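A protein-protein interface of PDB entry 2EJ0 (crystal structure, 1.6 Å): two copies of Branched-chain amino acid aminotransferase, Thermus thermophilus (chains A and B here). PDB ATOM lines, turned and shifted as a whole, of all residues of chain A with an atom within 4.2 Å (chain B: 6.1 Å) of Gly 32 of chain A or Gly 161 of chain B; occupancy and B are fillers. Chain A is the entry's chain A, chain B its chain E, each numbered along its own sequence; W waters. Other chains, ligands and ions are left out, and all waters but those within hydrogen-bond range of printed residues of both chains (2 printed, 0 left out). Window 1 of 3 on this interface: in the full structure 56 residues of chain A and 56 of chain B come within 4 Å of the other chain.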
ATOM      1  N   ALA A  28      23.833  34.170 -14.146  1.00  0.00           N
ATOM      2  CA  ALA A  28      24.021  33.712 -12.769  1.00  0.00           C
ATOM      3  C   ALA A  28      24.128  32.201 -12.609  1.00  0.00           C
ATOM      4  O   ALA A  28      24.760  31.720 -11.671  1.00  0.00           O
ATOM      5  CB  ALA A  28      22.889  34.247 -11.883  1.00  0.00           C
ATOM      6  N   HIS A  30      25.649  30.279 -14.620  1.00  0.00           N
ATOM      7  CA  HIS A  30      26.963  29.903 -15.123  1.00  0.00           C
ATOM      8  C   HIS A  30      28.130  30.532 -14.373  1.00  0.00           C
ATOM      9  O   HIS A  30      29.187  29.915 -14.239  1.00  0.00           O
ATOM     10  CB  HIS A  30      27.098  30.303 -16.597  1.00  0.00           C
ATOM     11  CG  HIS A  30      26.129  29.620 -17.509  1.00  0.00           C
ATOM     12  ND1 HIS A  30      26.532  28.830 -18.564  1.00  0.00           N
ATOM     13  CD2 HIS A  30      24.775  29.619 -17.533  1.00  0.00           C
ATOM     14  CE1 HIS A  30      25.468  28.372 -19.199  1.00  0.00           C
ATOM     15  NE2 HIS A  30      24.390  28.836 -18.593  1.00  0.00           N
ATOM     16  N   TYR A  31      27.931  31.748 -13.872  1.00  0.00           N
ATOM     17  CA  TYR A  31      29.017  32.485 -13.233  1.00  0.00           C
ATOM     18  C   TYR A  31      28.819  32.968 -11.799  1.00  0.00           C
ATOM     19  O   TYR A  31      29.606  33.786 -11.314  1.00  0.00           O
ATOM     20  CB  TYR A  31      29.372  33.681 -14.124  1.00  0.00           C
ATOM     21  CG  TYR A  31      29.583  33.326 -15.588  1.00  0.00           C
ATOM     22  CD1 TYR A  31      28.861  33.976 -16.591  1.00  0.00           C
ATOM     23  CD2 TYR A  31      30.522  32.369 -15.970  1.00  0.00           C
ATOM     24  CE1 TYR A  31      29.071  33.682 -17.939  1.00  0.00           C
ATOM     25  CE2 TYR A  31      30.740  32.065 -17.316  1.00  0.00           C
ATOM     26  CZ  TYR A  31      30.011  32.726 -18.294  1.00  0.00           C
ATOM     27  OH  TYR A  31      30.229  32.438 -19.624  1.00  0.00           O
ATOM     28  N   GLY A  32      27.772  32.482 -11.135  1.00  0.00           N
ATOM     29  CA  GLY A  32      27.505  32.850  -9.748  1.00  0.00           C
ATOM     30  C   GLY A  32      27.130  34.298  -9.480  1.00  0.00           C
ATOM     31  O   GLY A  32      27.163  34.761  -8.336  1.00  0.00           O
ATOM     32  N   THR A  33      26.732  35.002 -10.532  1.00  0.00           N
ATOM     33  CA  THR A  33      26.384  36.413 -10.440  1.00  0.00           C
ATOM     34  C   THR A  33      24.965  36.718  -9.972  1.00  0.00           C
ATOM     35  O   THR A  33      24.139  37.250 -10.722  1.00  0.00           O
ATOM     36  CB  THR A  33      26.643  37.079 -11.791  1.00  0.00           C
ATOM     37  OG1 THR A  33      26.141  36.229 -12.830  1.00  0.00           O
ATOM     38  CG2 THR A  33      28.147  37.271 -11.997  1.00  0.00           C
ATOM     39  N   SER A  34      24.699  36.377  -8.719  1.00  0.00           N
ATOM     40  CA  SER A  34      23.404  36.627  -8.104  1.00  0.00           C
ATOM     41  C   SER A  34      23.660  37.154  -6.700  1.00  0.00           C
ATOM     42  O   SER A  34      24.775  37.060  -6.189  1.00  0.00           O
ATOM     43  CB  SER A  34      22.587  35.331  -8.015  1.00  0.00           C
ATOM     44  OG  SER A  34      23.227  34.377  -7.174  1.00  0.00           O
ATOM     45  N   VAL A 160      26.780  37.317  -2.272  1.00  0.00           N
ATOM     46  CA  VAL A 160      26.876  37.039  -3.699  1.00  0.00           C
ATOM     47  C   VAL A 160      26.860  35.524  -3.862  1.00  0.00           C
ATOM     48  O   VAL A 160      27.575  34.810  -3.163  1.00  0.00           O
ATOM     49  CB  VAL A 160      28.182  37.626  -4.292  1.00  0.00           C
ATOM     50  CG1 VAL A 160      28.399  37.124  -5.720  1.00  0.00           C
ATOM     51  CG2 VAL A 160      28.103  39.147  -4.280  1.00  0.00           C
ATOM     52  N   GLY A 161      26.028  35.044  -4.780  1.00  0.00           N
ATOM     53  CA  GLY A 161      25.904  33.617  -5.013  1.00  0.00           C
ATOM     54  C   GLY A 161      27.205  32.843  -5.077  1.00  0.00           C
ATOM     55  O   GLY A 161      27.372  31.851  -4.372  1.00  0.00           O
ATOM     56  N   GLY A 162      28.126  33.295  -5.922  1.00  0.00           N
ATOM     57  CA  GLY A 162      29.399  32.612  -6.065  1.00  0.00           C
ATOM     58  C   GLY A 162      30.161  32.399  -4.768  1.00  0.00           C
ATOM     59  O   GLY A 162      30.868  31.402  -4.620  1.00  0.00           O
ATOM     60  N   ALA B  28      22.056  26.158  -7.603  1.00  0.00           N
ATOM     61  CA  ALA B  28      23.103  26.861  -8.341  1.00  0.00           C
ATOM     62  C   ALA B  28      22.824  28.340  -8.598  1.00  0.00           C
ATOM     63  O   ALA B  28      23.756  29.128  -8.743  1.00  0.00           O
ATOM     64  CB  ALA B  28      23.377  26.145  -9.662  1.00  0.00           C
ATOM     65  N   TYR B  31      23.734  29.684  -4.937  1.00  0.00           N
ATOM     66  CA  TYR B  31      25.048  29.411  -4.368  1.00  0.00           C
ATOM     67  C   TYR B  31      26.213  29.114  -5.317  1.00  0.00           C
ATOM     68  O   TYR B  31      27.262  28.648  -4.872  1.00  0.00           O
ATOM     69  CB  TYR B  31      24.903  28.260  -3.364  1.00  0.00           C
ATOM     70  CG  TYR B  31      23.769  28.449  -2.366  1.00  0.00           C
ATOM     71  CD1 TYR B  31      22.763  27.491  -2.234  1.00  0.00           C
ATOM     72  CD2 TYR B  31      23.713  29.577  -1.546  1.00  0.00           C
ATOM     73  CE1 TYR B  31      21.729  27.650  -1.303  1.00  0.00           C
ATOM     74  CE2 TYR B  31      22.684  29.743  -0.614  1.00  0.00           C
ATOM     75  CZ  TYR B  31      21.699  28.778  -0.499  1.00  0.00           C
ATOM     76  OH  TYR B  31      20.689  28.935   0.432  1.00  0.00           O
ATOM     77  N   GLY B  32      26.028  29.375  -6.609  1.00  0.00           N
ATOM     78  CA  GLY B  32      27.089  29.167  -7.588  1.00  0.00           C
ATOM     79  C   GLY B  32      27.546  27.739  -7.805  1.00  0.00           C
ATOM     80  O   GLY B  32      28.607  27.488  -8.379  1.00  0.00           O
ATOM     81  N   THR B  33      26.720  26.798  -7.376  1.00  0.00           N
ATOM     82  CA  THR B  33      27.036  25.386  -7.481  1.00  0.00           C
ATOM     83  C   THR B  33      26.730  24.750  -8.833  1.00  0.00           C
ATOM     84  O   THR B  33      25.851  23.893  -8.959  1.00  0.00           O
ATOM     85  CB  THR B  33      26.313  24.627  -6.372  1.00  0.00           C
ATOM     86  OG1 THR B  33      24.959  25.088  -6.300  1.00  0.00           O
ATOM     87  CG2 THR B  33      26.998  24.877  -5.034  1.00  0.00           C
ATOM     88  N   SER B  34      27.468  25.185  -9.846  1.00  0.00           N
ATOM     89  CA  SER B  34      27.324  24.643 -11.190  1.00  0.00           C
ATOM     90  C   SER B  34      28.720  24.442 -11.749  1.00  0.00           C
ATOM     91  O   SER B  34      29.693  24.950 -11.196  1.00  0.00           O
ATOM     92  CB  SER B  34      26.559  25.619 -12.091  1.00  0.00           C
ATOM     93  OG  SER B  34      27.267  26.842 -12.246  1.00  0.00           O
ATOM     94  N   VAL B  35      28.820  23.668 -12.823  1.00  0.00           N
ATOM     95  CA  VAL B  35      30.099  23.460 -13.495  1.00  0.00           C
ATOM     96  C   VAL B  35      29.783  23.573 -14.978  1.00  0.00           C
ATOM     97  O   VAL B  35      28.664  23.277 -15.404  1.00  0.00           O
ATOM     98  CB  VAL B  35      30.731  22.067 -13.206  1.00  0.00           C
ATOM     99  CG1 VAL B  35      31.014  21.918 -11.722  1.00  0.00           C
ATOM    100  CG2 VAL B  35      29.814  20.956 -13.694  1.00  0.00           C
ATOM    101  N   PHE B  36      30.753  24.014 -15.767  1.00  0.00           N
ATOM    102  CA  PHE B  36      30.512  24.164 -17.191  1.00  0.00           C
ATOM    103  C   PHE B  36      31.780  24.000 -17.995  1.00  0.00           C
ATOM    104  O   PHE B  36      32.867  23.839 -17.443  1.00  0.00           O
ATOM    105  CB  PHE B  36      29.884  25.537 -17.478  1.00  0.00           C
ATOM    106  CG  PHE B  36      30.801  26.712 -17.215  1.00  0.00           C
ATOM    107  CD1 PHE B  36      31.617  27.222 -18.225  1.00  0.00           C
ATOM    108  CD2 PHE B  36      30.826  27.325 -15.966  1.00  0.00           C
ATOM    109  CE1 PHE B  36      32.441  28.328 -17.996  1.00  0.00           C
ATOM    110  CE2 PHE B  36      31.646  28.430 -15.724  1.00  0.00           C
ATOM    111  CZ  PHE B  36      32.454  28.933 -16.743  1.00  0.00           C
ATOM    112  N   LEU B  67      32.958  19.370  -6.651  1.00  0.00           N
ATOM    113  CA  LEU B  67      31.765  19.753  -5.897  1.00  0.00           C
ATOM    114  C   LEU B  67      31.010  18.529  -5.395  1.00  0.00           C
ATOM    115  O   LEU B  67      29.943  18.661  -4.799  1.00  0.00           O
ATOM    116  CB  LEU B  67      30.812  20.572  -6.770  1.00  0.00           C
ATOM    117  CG  LEU B  67      31.190  21.995  -7.172  1.00  0.00           C
ATOM    118  CD1 LEU B  67      30.069  22.582  -8.015  1.00  0.00           C
ATOM    119  CD2 LEU B  67      31.418  22.841  -5.929  1.00  0.00           C
ATOM    120  N   LYS B 159      35.962  24.412 -13.468  1.00  0.00           N
ATOM    121  CA  LYS B 159      35.165  25.506 -13.992  1.00  0.00           C
ATOM    122  C   LYS B 159      33.852  25.489 -13.219  1.00  0.00           C
ATOM    123  O   LYS B 159      32.806  25.097 -13.737  1.00  0.00           O
ATOM    124  CB  LYS B 159      34.923  25.342 -15.498  1.00  0.00           C
ATOM    125  CG  LYS B 159      36.209  25.378 -16.314  1.00  0.00           C
ATOM    126  CD  LYS B 159      35.963  25.393 -17.820  1.00  0.00           C
ATOM    127  CE  LYS B 159      35.484  26.749 -18.304  1.00  0.00           C
ATOM    128  NZ  LYS B 159      35.481  26.828 -19.795  1.00  0.00           N
ATOM    129  N   VAL B 160      33.943  25.882 -11.953  1.00  0.00           N
ATOM    130  CA  VAL B 160      32.791  25.954 -11.062  1.00  0.00           C
ATOM    131  C   VAL B 160      32.188  27.347 -11.200  1.00  0.00           C
ATOM    132  O   VAL B 160      32.899  28.352 -11.154  1.00  0.00           O
ATOM    133  CB  VAL B 160      33.211  25.700  -9.593  1.00  0.00           C
ATOM    134  CG1 VAL B 160      32.080  26.074  -8.646  1.00  0.00           C
ATOM    135  CG2 VAL B 160      33.578  24.233  -9.414  1.00  0.00           C
ATOM    136  N   GLY B 161      30.873  27.399 -11.382  1.00  0.00           N
ATOM    137  CA  GLY B 161      30.194  28.671 -11.558  1.00  0.00           C
ATOM    138  C   GLY B 161      30.607  29.784 -10.613  1.00  0.00           C
ATOM    139  O   GLY B 161      30.954  30.879 -11.057  1.00  0.00           O
ATOM    140  N   GLY B 162      30.576  29.508  -9.313  1.00  0.00           N
ATOM    141  CA  GLY B 162      30.936  30.518  -8.329  1.00  0.00           C
ATOM    142  C   GLY B 162      32.304  31.146  -8.530  1.00  0.00           C
ATOM    143  O   GLY B 162      32.508  32.317  -8.200  1.00  0.00           O
ATOM    144  N   ASN B 163      33.242  30.368  -9.061  1.00  0.00           N
ATOM    145  CA  ASN B 163      34.597  30.849  -9.311  1.00  0.00           C
ATOM    146  C   ASN B 163      34.586  32.107 -10.158  1.00  0.00           C
ATOM    147  O   ASN B 163      35.406  33.009  -9.969  1.00  0.00           O
ATOM    148  CB  ASN B 163      35.411  29.815 -10.091  1.00  0.00           C
ATOM    149  CG  ASN B 163      35.783  28.599  -9.278  1.00  0.00           C
ATOM    150  OD1 ASN B 163      35.334  28.413  -8.148  1.00  0.00           O
ATOM    151  ND2 ASN B 163      36.615  27.749  -9.866  1.00  0.00           N
ATOM    152  N   TYR B 164      33.646  32.166 -11.096  1.00  0.00           N
ATOM    153  CA  TYR B 164      33.602  33.277 -12.026  1.00  0.00           C
ATOM    154  C   TYR B 164      33.129  34.632 -11.531  1.00  0.00           C
ATOM    155  O   TYR B 164      33.071  35.596 -12.291  1.00  0.00           O
ATOM    156  CB  TYR B 164      32.889  32.818 -13.302  1.00  0.00           C
ATOM    157  CG  TYR B 164      33.730  31.765 -13.993  1.00  0.00           C
ATOM    158  CD1 TYR B 164      33.745  30.446 -13.532  1.00  0.00           C
ATOM    159  CD2 TYR B 164      34.621  32.113 -15.010  1.00  0.00           C
ATOM    160  CE1 TYR B 164      34.631  29.505 -14.053  1.00  0.00           C
ATOM    161  CE2 TYR B 164      35.515  31.180 -15.539  1.00  0.00           C
ATOM    162  CZ  TYR B 164      35.515  29.881 -15.052  1.00  0.00           C
ATOM    163  OH  TYR B 164      36.420  28.963 -15.535  1.00  0.00           O
ATOM    164  N   VAL B 165      32.809  34.716 -10.247  1.00  0.00           N
ATOM    165  CA  VAL B 165      32.445  36.000  -9.671  1.00  0.00           C
ATOM    166  C   VAL B 165      33.777  36.758  -9.636  1.00  0.00           C
ATOM    167  O   VAL B 165      33.836  37.958  -9.900  1.00  0.00           O
ATOM    168  CB  VAL B 165      31.891  35.830  -8.241  1.00  0.00           C
ATOM    169  CG1 VAL B 165      31.964  37.147  -7.482  1.00  0.00           C
ATOM    170  CG2 VAL B 165      30.451  35.339  -8.310  1.00  0.00           C
HETATM  171  O   HOH W   1      24.836  31.757  -8.167  1.00  0.00           O
HETATM  172  O   HOH W   2      26.590  29.657 -10.777  1.00  0.00           O
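O of Gly 161 of chain B lies close to O of Tyr 31 of chain A (3.2 Å).
The backbone carbonyl oxygen of Gly 161 of chain A lies close to the backbone carbonyl oxygen of Tyr 31 of chain B, 3.2 Å away.
The backbone carbonyl oxygen of Gly 32 of chain A lies within hydrogen-bond range of the backbone NH of Gly 162 of chain A (3.0 Å).
The backbone carbonyl oxygen (O) of Ser 34 of chain A sits at hydrogen-bond distance from the backbone NH (N) of Gly 161 of chain A (2.8 Å).
O of Gly 32 of chain B is in hydrogen-bond range of N of Gly 162 of chain B, at 3.0 Å.
O of Ser 34 of chain B is in hydrogen-bond range of N of Gly 161 of chain B, 2.7 Å away.
N of Phe 36 of chain B sits at hydrogen-bond distance from O of Lys 159 of chain B (3.1 Å).
Phe 36 of chain B touches His 30 of chain A (CE2 to O, 3.2 Å).
His 30 of chain A touches Gly 161 of chain B.
Tyr 31 of chain A touches Phe 36 of chain B.
CB of Tyr 164 of chain B touches CD2 of Tyr 31 of chain A (3.6 Å).
CG2 of Val 165 of chain B touches O of Tyr 31 of chain A, at 3.5 Å.
Gly 161 of chain B touches Gly 32 of chain A.
Gly 32 of chain A touches Val 165 of chain B.
N of Gly 32 of chain B touches O of Gly 161 of chain A, at 3.6 Å.
Gly 162 of chain B touches Gly 162 of chain A (CA to CA, 3.4 Å).
Gly 162 of chain A touches Val 165 of chain B (CA to CG2, 3.7 Å).
Gly 161 of chain B touches three residues of chain A.
Printed residues of chain A within 4 Å of Gly 162 of chain B: Gly 162.
Printed residues of chain B within 4 Å of Val 160 of chain A: Val 165 (3.8 Å).
Of the printed residues of chain A, Tyr 31 of chain B touches Gly 161 (3.1 Å).
The nearest printed residue of chain A that does not touch Gly 161 of chain B is Gly 162 of chain A (5.5 Å).
The nearest printed residue of chain B that does not touch Gly 162 of chain A is Gly 32 of chain B (4.4 Å).
Hydrophobic or aromatic side chains of chain A within 4 Å of the printed part of chain B: Tyr 31 and Val 160.
Along chain B the printed residues that touch a printed residue of chain A span positions 31 to 165.
Tyr 31 of chain A touches Gly 161 of chain B, and with the chains exchanged Gly 161 of chain A touches Tyr 31 of chain B.
Gly 32 of chain A touches Gly 161 of chain B, and with the chains exchanged Gly 161 of chain A touches Gly 32 of chain B.
Gly 162 of chain B touches its own counterpart, Gly 162 of chain A.
Positions printed for both chains: 28, 31, 32, 33, 34, 160, 161 and 162.
Water W2 lies within hydrogen-bond range of O of Ala 28 of chain A (2.9 Å), N of Gly 32 of chain A (3.1 Å) and OG of Ser 34 of chain B (3.2 Å).
Water W1 lies within hydrogen-bond range of the backbone carbonyl oxygen of Ala 28 of chain B (2.9 Å), the backbone NH of Gly 32 of chain B (3.1 Å) and the side-chain hydroxyl of Ser 34 of chain A (3.2 Å).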
